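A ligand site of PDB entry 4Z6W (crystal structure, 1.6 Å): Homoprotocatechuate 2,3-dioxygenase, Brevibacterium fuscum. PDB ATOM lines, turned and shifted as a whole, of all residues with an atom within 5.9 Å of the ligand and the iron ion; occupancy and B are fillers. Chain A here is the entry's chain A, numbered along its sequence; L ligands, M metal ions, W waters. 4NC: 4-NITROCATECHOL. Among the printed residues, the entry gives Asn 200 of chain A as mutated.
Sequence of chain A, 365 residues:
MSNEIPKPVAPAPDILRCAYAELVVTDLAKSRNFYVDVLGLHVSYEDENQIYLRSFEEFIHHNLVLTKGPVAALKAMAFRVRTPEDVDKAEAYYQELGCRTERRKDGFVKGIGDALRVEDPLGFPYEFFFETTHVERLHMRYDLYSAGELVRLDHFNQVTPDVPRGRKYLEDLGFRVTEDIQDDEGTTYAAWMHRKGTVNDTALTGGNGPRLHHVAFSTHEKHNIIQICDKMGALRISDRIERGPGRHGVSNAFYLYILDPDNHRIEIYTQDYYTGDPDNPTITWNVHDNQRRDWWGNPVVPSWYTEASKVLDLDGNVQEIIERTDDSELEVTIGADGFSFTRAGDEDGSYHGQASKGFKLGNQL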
ATOM      1  N   HIS A 155      35.262  -7.709  -2.184  1.00  0.00           N
ATOM      2  CA  HIS A 155      35.938  -8.640  -3.118  1.00  0.00           C
ATOM      3  C   HIS A 155      35.833  -8.248  -4.560  1.00  0.00           C
ATOM      4  O   HIS A 155      35.047  -7.391  -4.932  1.00  0.00           O
ATOM      5  CB  HIS A 155      35.416 -10.083  -2.915  1.00  0.00           C
ATOM      6  CG  HIS A 155      33.979 -10.315  -3.286  1.00  0.00           C
ATOM      7  ND1 HIS A 155      32.958 -10.292  -2.373  1.00  0.00           N
ATOM      8  CD2 HIS A 155      33.410 -10.643  -4.474  1.00  0.00           C
ATOM      9  CE1 HIS A 155      31.810 -10.611  -2.970  1.00  0.00           C
ATOM     10  NE2 HIS A 155      32.059 -10.797  -4.248  1.00  0.00           N
ATOM     11  N   PHE A 156      36.613  -8.957  -5.350  1.00  0.00           N
ATOM     12  CA  PHE A 156      36.523  -8.967  -6.793  1.00  0.00           C
ATOM     13  C   PHE A 156      36.040 -10.344  -7.266  1.00  0.00           C
ATOM     14  O   PHE A 156      36.186 -11.338  -6.543  1.00  0.00           O
ATOM     15  CB  PHE A 156      37.911  -8.741  -7.408  1.00  0.00           C
ATOM     16  CG  PHE A 156      38.667  -7.557  -6.847  1.00  0.00           C
ATOM     17  CD1 PHE A 156      38.087  -6.282  -6.811  1.00  0.00           C
ATOM     18  CD2 PHE A 156      39.979  -7.720  -6.403  1.00  0.00           C
ATOM     19  CE1 PHE A 156      38.810  -5.189  -6.323  1.00  0.00           C
ATOM     20  CE2 PHE A 156      40.695  -6.636  -5.905  1.00  0.00           C
ATOM     21  CZ  PHE A 156      40.122  -5.384  -5.876  1.00  0.00           C
ATOM     22  N   ASN A 157      35.550 -10.411  -8.495  1.00  0.00           N
ATOM     23  CA  ASN A 157      35.239 -11.718  -9.111  1.00  0.00           C
ATOM     24  C   ASN A 157      35.646 -11.637 -10.592  1.00  0.00           C
ATOM     25  O   ASN A 157      35.226 -10.748 -11.307  1.00  0.00           O
ATOM     26  CB  ASN A 157      33.740 -12.011  -8.965  1.00  0.00           C
ATOM     27  CG  ASN A 157      33.372 -13.391  -9.447  1.00  0.00           C
ATOM     28  OD1 ASN A 157      33.607 -13.726 -10.592  1.00  0.00           O
ATOM     29  ND2 ASN A 157      32.770 -14.196  -8.565  1.00  0.00           N
ATOM     30  N   ILE A 181      32.152 -24.675  -7.027  1.00  0.00           N
ATOM     31  CA  ILE A 181      31.067 -25.333  -7.717  1.00  0.00           C
ATOM     32  C   ILE A 181      31.664 -26.298  -8.733  1.00  0.00           C
ATOM     33  O   ILE A 181      32.497 -25.911  -9.574  1.00  0.00           O
ATOM     34  CB  ILE A 181      30.153 -24.324  -8.427  1.00  0.00           C
ATOM     35  CG1 ILE A 181      29.424 -23.401  -7.427  1.00  0.00           C
ATOM     36  CG2 ILE A 181      29.128 -25.054  -9.293  1.00  0.00           C
ATOM     37  CD1 ILE A 181      28.652 -22.241  -8.060  1.00  0.00           C
ATOM     38  N   TRP A 192      35.973 -19.618  -4.980  1.00  0.00           N
ATOM     39  CA  TRP A 192      36.124 -18.441  -4.160  1.00  0.00           C
ATOM     40  C   TRP A 192      37.313 -18.612  -3.257  1.00  0.00           C
ATOM     41  O   TRP A 192      37.506 -19.686  -2.683  1.00  0.00           O
ATOM     42  CB  TRP A 192      34.871 -18.228  -3.328  1.00  0.00           C
ATOM     43  CG  TRP A 192      33.642 -17.727  -4.117  1.00  0.00           C
ATOM     44  CD1 TRP A 192      33.174 -16.439  -4.178  1.00  0.00           C
ATOM     45  CD2 TRP A 192      32.789 -18.499  -4.967  1.00  0.00           C
ATOM     46  NE1 TRP A 192      32.093 -16.368  -5.011  1.00  0.00           N
ATOM     47  CE2 TRP A 192      31.835 -17.613  -5.514  1.00  0.00           C
ATOM     48  CE3 TRP A 192      32.724 -19.853  -5.313  1.00  0.00           C
ATOM     49  CZ2 TRP A 192      30.813 -18.040  -6.366  1.00  0.00           C
ATOM     50  CZ3 TRP A 192      31.716 -20.273  -6.193  1.00  0.00           C
ATOM     51  CH2 TRP A 192      30.774 -19.361  -6.693  1.00  0.00           C
ATOM     52  N   VAL A 199      34.710 -14.938   3.005  1.00  0.00           N
ATOM     53  CA  VAL A 199      34.583 -15.985   1.982  1.00  0.00           C
ATOM     54  C   VAL A 199      35.480 -15.712   0.754  1.00  0.00           C
ATOM     55  O   VAL A 199      35.983 -16.662   0.173  1.00  0.00           O
ATOM     56  CB  VAL A 199      33.085 -16.188   1.617  1.00  0.00           C
ATOM     57  CG1 VAL A 199      32.932 -17.103   0.403  1.00  0.00           C
ATOM     58  CG2 VAL A 199      32.426 -16.835   2.790  1.00  0.00           C
ATOM     59  N   ASN A 200      35.748 -14.436   0.431  1.00  0.00           N
ATOM     60  CA  ASN A 200      36.373 -14.066  -0.855  1.00  0.00           C
ATOM     61  C   ASN A 200      37.172 -12.770  -0.694  1.00  0.00           C
ATOM     62  O   ASN A 200      36.690 -11.819  -0.051  1.00  0.00           O
ATOM     63  CB  ASN A 200      35.298 -13.910  -1.938  1.00  0.00           C
ATOM     64  CG  ASN A 200      35.856 -14.005  -3.349  1.00  0.00           C
ATOM     65  OD1 ASN A 200      35.428 -13.302  -4.249  1.00  0.00           O
ATOM     66  ND2 ASN A 200      36.834 -14.850  -3.516  1.00  0.00           N
ATOM     67  N   HIS A 213      34.149  -9.885 -13.641  1.00  0.00           N
ATOM     68  CA  HIS A 213      32.753 -10.120 -13.426  1.00  0.00           C
ATOM     69  C   HIS A 213      32.118  -9.007 -12.584  1.00  0.00           C
ATOM     70  O   HIS A 213      31.144  -8.446 -13.009  1.00  0.00           O
ATOM     71  CB  HIS A 213      32.489 -11.496 -12.805  1.00  0.00           C
ATOM     72  CG  HIS A 213      31.076 -11.914 -12.971  1.00  0.00           C
ATOM     73  ND1 HIS A 213      30.083 -11.402 -12.176  1.00  0.00           N
ATOM     74  CD2 HIS A 213      30.455 -12.669 -13.905  1.00  0.00           C
ATOM     75  CE1 HIS A 213      28.914 -11.872 -12.567  1.00  0.00           C
ATOM     76  NE2 HIS A 213      29.108 -12.617 -13.636  1.00  0.00           N
ATOM     77  N   HIS A 214      32.654  -8.743 -11.393  1.00  0.00           N
ATOM     78  CA  HIS A 214      32.162  -7.663 -10.569  1.00  0.00           C
ATOM     79  C   HIS A 214      33.132  -7.273  -9.509  1.00  0.00           C
ATOM     80  O   HIS A 214      34.110  -7.961  -9.278  1.00  0.00           O
ATOM     81  CB  HIS A 214      30.791  -8.051  -9.959  1.00  0.00           C
ATOM     82  CG  HIS A 214      30.816  -9.269  -9.064  1.00  0.00           C
ATOM     83  ND1 HIS A 214      30.538 -10.531  -9.530  1.00  0.00           N
ATOM     84  CD2 HIS A 214      31.018  -9.412  -7.740  1.00  0.00           C
ATOM     85  CE1 HIS A 214      30.585 -11.404  -8.552  1.00  0.00           C
ATOM     86  NE2 HIS A 214      30.901 -10.753  -7.451  1.00  0.00           N
ATOM     87  N   ALA A 216      32.576  -6.054  -5.441  1.00  0.00           N
ATOM     88  CA  ALA A 216      31.564  -6.145  -4.420  1.00  0.00           C
ATOM     89  C   ALA A 216      31.880  -5.214  -3.262  1.00  0.00           C
ATOM     90  O   ALA A 216      33.019  -5.214  -2.734  1.00  0.00           O
ATOM     91  CB  ALA A 216      31.501  -7.557  -3.880  1.00  0.00           C
ATOM     92  N   ARG A 243      20.140  -8.637 -10.971  1.00  0.00           N
ATOM     93  CA  ARG A 243      19.874  -9.912 -10.293  1.00  0.00           C
ATOM     94  C   ARG A 243      19.784  -9.629  -8.799  1.00  0.00           C
ATOM     95  O   ARG A 243      20.607  -8.927  -8.235  1.00  0.00           O
ATOM     96  CB  ARG A 243      20.956 -10.937 -10.612  1.00  0.00           C
ATOM     97  CG  ARG A 243      20.983 -12.185  -9.747  1.00  0.00           C
ATOM     98  CD  ARG A 243      21.914 -13.302 -10.237  1.00  0.00           C
ATOM     99  NE  ARG A 243      21.895 -14.276  -9.149  1.00  0.00           N
ATOM    100  CZ  ARG A 243      22.949 -14.858  -8.605  1.00  0.00           C
ATOM    101  NH1 ARG A 243      24.154 -14.790  -9.120  1.00  0.00           N
ATOM    102  NH2 ARG A 243      22.754 -15.599  -7.537  1.00  0.00           N
ATOM    103  N   HIS A 248      22.680 -15.781  -1.159  1.00  0.00           N
ATOM    104  CA  HIS A 248      23.512 -16.708  -1.893  1.00  0.00           C
ATOM    105  C   HIS A 248      23.520 -18.078  -1.189  1.00  0.00           C
ATOM    106  O   HIS A 248      23.417 -18.135   0.065  1.00  0.00           O
ATOM    107  CB  HIS A 248      24.985 -16.246  -1.921  1.00  0.00           C
ATOM    108  CG  HIS A 248      25.278 -15.173  -2.909  1.00  0.00           C
ATOM    109  ND1 HIS A 248      24.918 -15.264  -4.225  1.00  0.00           N
ATOM    110  CD2 HIS A 248      25.987 -14.024  -2.784  1.00  0.00           C
ATOM    111  CE1 HIS A 248      25.374 -14.207  -4.880  1.00  0.00           C
ATOM    112  NE2 HIS A 248      26.019 -13.444  -4.024  1.00  0.00           N
ATOM    113  N   GLY A 249      23.687 -19.157  -1.935  1.00  0.00           N
ATOM    114  CA  GLY A 249      24.112 -20.418  -1.333  1.00  0.00           C
ATOM    115  C   GLY A 249      25.573 -20.360  -0.995  1.00  0.00           C
ATOM    116  O   GLY A 249      25.913 -20.285   0.164  1.00  0.00           O
ATOM    117  N   VAL A 250      26.429 -20.399  -2.014  1.00  0.00           N
ATOM    118  CA  VAL A 250      27.842 -20.139  -1.838  1.00  0.00           C
ATOM    119  C   VAL A 250      28.000 -18.793  -1.090  1.00  0.00           C
ATOM    120  O   VAL A 250      27.445 -17.805  -1.510  1.00  0.00           O
ATOM    121  CB  VAL A 250      28.546 -19.999  -3.196  1.00  0.00           C
ATOM    122  CG1 VAL A 250      29.953 -19.455  -2.997  1.00  0.00           C
ATOM    123  CG2 VAL A 250      28.608 -21.327  -3.967  1.00  0.00           C
ATOM    124  N   SER A 251      28.705 -18.817   0.034  1.00  0.00           N
ATOM    125  CA  SER A 251      29.025 -17.630   0.866  1.00  0.00           C
ATOM    126  C   SER A 251      27.974 -17.313   1.920  1.00  0.00           C
ATOM    127  O   SER A 251      28.290 -16.656   2.914  1.00  0.00           O
ATOM    128  CB  SER A 251      29.326 -16.338   0.060  1.00  0.00           C
ATOM    129  OG  SER A 251      28.124 -15.650  -0.258  1.00  0.00           O
ATOM    130  N   TYR A 257      22.942  -7.466  -7.391  1.00  0.00           N
ATOM    131  CA  TYR A 257      23.845  -7.063  -8.529  1.00  0.00           C
ATOM    132  C   TYR A 257      23.184  -5.959  -9.341  1.00  0.00           C
ATOM    133  O   TYR A 257      22.040  -6.099  -9.776  1.00  0.00           O
ATOM    134  CB  TYR A 257      24.139  -8.233  -9.467  1.00  0.00           C
ATOM    135  CG  TYR A 257      24.872  -9.381  -8.839  1.00  0.00           C
ATOM    136  CD1 TYR A 257      26.258  -9.391  -8.730  1.00  0.00           C
ATOM    137  CD2 TYR A 257      24.185 -10.435  -8.306  1.00  0.00           C
ATOM    138  CE1 TYR A 257      26.924 -10.435  -8.102  1.00  0.00           C
ATOM    139  CE2 TYR A 257      24.855 -11.489  -7.698  1.00  0.00           C
ATOM    140  CZ  TYR A 257      26.212 -11.479  -7.612  1.00  0.00           C
ATOM    141  OH  TYR A 257      26.829 -12.556  -7.056  1.00  0.00           O
ATOM    142  N   GLU A 267      28.390  -5.710  -7.131  1.00  0.00           N
ATOM    143  CA  GLU A 267      27.652  -6.460  -6.122  1.00  0.00           C
ATOM    144  C   GLU A 267      27.588  -5.705  -4.810  1.00  0.00           C
ATOM    145  O   GLU A 267      28.578  -5.109  -4.379  1.00  0.00           O
ATOM    146  CB  GLU A 267      28.289  -7.810  -5.862  1.00  0.00           C
ATOM    147  CG  GLU A 267      27.435  -8.776  -5.046  1.00  0.00           C
ATOM    148  CD  GLU A 267      28.076 -10.108  -4.753  1.00  0.00           C
ATOM    149  OE1 GLU A 267      29.272 -10.289  -5.062  1.00  0.00           O
ATOM    150  OE2 GLU A 267      27.363 -11.015  -4.262  1.00  0.00           O
ATOM    151  N   TYR A 269      26.698  -6.692  -0.836  1.00  0.00           N
ATOM    152  CA  TYR A 269      26.961  -7.990  -0.198  1.00  0.00           C
ATOM    153  C   TYR A 269      26.988  -7.817   1.306  1.00  0.00           C
ATOM    154  O   TYR A 269      27.504  -6.798   1.827  1.00  0.00           O
ATOM    155  CB  TYR A 269      28.311  -8.480  -0.716  1.00  0.00           C
ATOM    156  CG  TYR A 269      28.859  -9.809  -0.331  1.00  0.00           C
ATOM    157  CD1 TYR A 269      28.654 -10.939  -1.122  1.00  0.00           C
ATOM    158  CD2 TYR A 269      29.724  -9.901   0.763  1.00  0.00           C
ATOM    159  CE1 TYR A 269      29.284 -12.122  -0.822  1.00  0.00           C
ATOM    160  CE2 TYR A 269      30.329 -11.098   1.086  1.00  0.00           C
ATOM    161  CZ  TYR A 269      30.107 -12.202   0.277  1.00  0.00           C
ATOM    162  OH  TYR A 269      30.762 -13.359   0.563  1.00  0.00           O
ATOM    163  N   ARG A 292      22.361 -23.244  -5.053  1.00  0.00           N
ATOM    164  CA  ARG A 292      23.786 -22.924  -4.886  1.00  0.00           C
ATOM    165  C   ARG A 292      24.105 -21.441  -5.084  1.00  0.00           C
ATOM    166  O   ARG A 292      25.002 -20.912  -4.427  1.00  0.00           O
ATOM    167  CB  ARG A 292      24.611 -23.761  -5.887  1.00  0.00           C
ATOM    168  CG  ARG A 292      24.599 -23.211  -7.292  1.00  0.00           C
ATOM    169  CD  ARG A 292      25.142 -24.168  -8.363  1.00  0.00           C
ATOM    170  NE  ARG A 292      25.037 -23.512  -9.650  1.00  0.00           N
ATOM    171  CZ  ARG A 292      23.890 -23.293 -10.314  1.00  0.00           C
ATOM    172  NH1 ARG A 292      22.721 -23.747  -9.835  1.00  0.00           N
ATOM    173  NH2 ARG A 292      23.890 -22.565 -11.414  1.00  0.00           N
ATOM    174  N   ARG A 293      23.398 -20.758  -5.984  1.00  0.00           N
ATOM    175  CA  ARG A 293      23.709 -19.350  -6.277  1.00  0.00           C
ATOM    176  C   ARG A 293      22.696 -18.438  -5.612  1.00  0.00           C
ATOM    177  O   ARG A 293      23.055 -17.426  -5.044  1.00  0.00           O
ATOM    178  CB  ARG A 293      23.801 -19.110  -7.772  1.00  0.00           C
ATOM    179  CG  ARG A 293      25.065 -19.704  -8.382  1.00  0.00           C
ATOM    180  CD  ARG A 293      25.480 -19.010  -9.642  1.00  0.00           C
ATOM    181  NE  ARG A 293      26.782 -19.506 -10.157  1.00  0.00           N
ATOM    182  CZ  ARG A 293      27.968 -19.015  -9.847  1.00  0.00           C
ATOM    183  NH1 ARG A 293      28.118 -18.008  -8.994  1.00  0.00           N
ATOM    184  NH2 ARG A 293      29.022 -19.493 -10.460  1.00  0.00           N
ATOM    185  N   ASP A 294      21.434 -18.766  -5.769  1.00  0.00           N
ATOM    186  CA  ASP A 294      20.366 -18.158  -4.966  1.00  0.00           C
ATOM    187  C   ASP A 294      19.730 -19.243  -4.143  1.00  0.00           C
ATOM    188  O   ASP A 294      19.158 -20.212  -4.678  1.00  0.00           O
ATOM    189  CB  ASP A 294      19.300 -17.523  -5.851  1.00  0.00           C
ATOM    190  CG  ASP A 294      18.324 -16.671  -5.049  1.00  0.00           C
ATOM    191  OD1 ASP A 294      18.685 -15.501  -4.717  1.00  0.00           O
ATOM    192  OD2 ASP A 294      17.219 -17.200  -4.703  1.00  0.00           O
ATOM    193  N   TRP A 304      23.917 -12.589 -16.405  1.00  0.00           N
ATOM    194  CA  TRP A 304      24.860 -12.706 -15.301  1.00  0.00           C
ATOM    195  C   TRP A 304      25.967 -13.663 -15.679  1.00  0.00           C
ATOM    196  O   TRP A 304      27.124 -13.549 -15.216  1.00  0.00           O
ATOM    197  CB  TRP A 304      24.083 -13.123 -14.039  1.00  0.00           C
ATOM    198  CG  TRP A 304      24.866 -12.948 -12.779  1.00  0.00           C
ATOM    199  CD1 TRP A 304      24.891 -11.845 -12.013  1.00  0.00           C
ATOM    200  CD2 TRP A 304      25.784 -13.865 -12.223  1.00  0.00           C
ATOM    201  NE1 TRP A 304      25.742 -12.035 -10.961  1.00  0.00           N
ATOM    202  CE2 TRP A 304      26.323 -13.264 -11.075  1.00  0.00           C
ATOM    203  CE3 TRP A 304      26.223 -15.143 -12.582  1.00  0.00           C
ATOM    204  CZ2 TRP A 304      27.283 -13.883 -10.275  1.00  0.00           C
ATOM    205  CZ3 TRP A 304      27.166 -15.756 -11.789  1.00  0.00           C
ATOM    206  CH2 TRP A 304      27.707 -15.112 -10.665  1.00  0.00           C
HETATM  207  C1  4NC L   1      29.492 -14.156  -4.499  1.00  0.00           C
HETATM  208  C2  4NC L   1      29.007 -14.080  -5.874  1.00  0.00           C
HETATM  209  C3  4NC L   1      28.286 -15.149  -6.429  1.00  0.00           C
HETATM  210  C4  4NC L   1      27.888 -16.184  -5.570  1.00  0.00           C
HETATM  211  C5  4NC L   1      28.345 -16.267  -4.269  1.00  0.00           C
HETATM  212  C6  4NC L   1      29.171 -15.313  -3.731  1.00  0.00           C
HETATM  213  O7  4NC L   1      30.154 -13.120  -3.965  1.00  0.00           O
HETATM  214  O8  4NC L   1      29.201 -13.021  -6.631  1.00  0.00           O
HETATM  215  N9  4NC L   1      26.942 -17.085  -6.018  1.00  0.00           N
HETATM  216  O10 4NC L   1      26.467 -17.992  -5.144  1.00  0.00           O
HETATM  217  O11 4NC L   1      26.065 -16.751  -7.058  1.00  0.00           O
HETATM  218 FE    FE M   1      30.563 -11.779  -5.517  1.00  0.00          FE
HETATM  219  O   HOH W   1      32.391 -13.375  -5.907  1.00  0.00           O
HETATM  220  O   HOH W   2      31.821 -14.003  -2.068  1.00  0.00           O
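Water W1 lies within hydrogen-bond range of ND2 of Asn 157 (2.8 Å), NE1 of Trp 192 (3.1 Å) and OD1 of Asn 200 (3.5 Å).
The side-chain hydroxyl (OH) of Tyr 257 lies close to an oxygen (O8) of the ligand.
The guanidinium group of Arg 293 sits at hydrogen-bond distance from an oxygen (O11) of the ligand, 3.1 Å away.
An oxygen (O10) of the ligand lies within hydrogen-bond range of a ring nitrogen (ND1) of His 248 (3.3 Å).
NH1 of Arg 243 is in hydrogen-bond range of O11 of the ligand, at 3.4 Å.
The side-chain carboxylate of Glu 267 lies within hydrogen-bond range of the side-chain hydroxyl of Tyr 257, 3.2 Å away.
The side-chain carboxylate (OE2) of Glu 267 lies within hydrogen-bond range of a ring nitrogen (NE2) of His 248 (2.8 Å).
O of His 155 is in hydrogen-bond range of N of Ala 216 (2.9 Å).
The backbone NH (N) of Asn 157 lies within hydrogen-bond range of the backbone carbonyl oxygen (O) of His 214, 2.9 Å away.
A ring nitrogen (NE2) of His 248 lies close to the side-chain hydroxyl of Tyr 257, at 3.3 Å.
The backbone carbonyl oxygen (O) of Arg 293 is in hydrogen-bond range of the guanidinium group (NH2) of Arg 243, 3.1 Å away.
N of Val 250 lies within hydrogen-bond range of O of Arg 292 (2.8 Å).
O of Arg 292 lies close to N of Gly 249.
The backbone carbonyl oxygen of Arg 292 lies close to an oxygen (O10) of the ligand (3.3 Å).
Trp 192 touches the ligand (NE1 to C6, 3.4 Å).
O of Val 250 touches C5 of the ligand, at 3.3 Å.
Ser 251 touches the ligand (OG to C6, 3.6 Å).
Tyr 269 touches the ligand (CE1 to O7, 3.4 Å).
Hydrophobic or aromatic side chains that line the ligand: His 155, Trp 192, His 214, His 248, Val 250, Tyr 257 and Tyr 269.
12 residues have an atom within 4 Å of the ligand: His 155, Trp 192, His 214, Arg 243, His 248, Val 250, Ser 251, Tyr 257, Glu 267, Tyr 269, Arg 292 and Arg 293.
The iron ion is bound by OE1 of Glu 267 (2.0 Å).
The iron ion is bound by O7 of the ligand (2.1 Å).
An oxygen (O8) of the ligand binds the iron ion (2.2 Å).
The iron ion is bound by NE2 of His 155.
A ring nitrogen (NE2) of His 214 binds the iron ion (2.2 Å).
Water W1 is bound to the iron ion (2.5 Å).
The iron ion has six donor atoms within binding distance.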
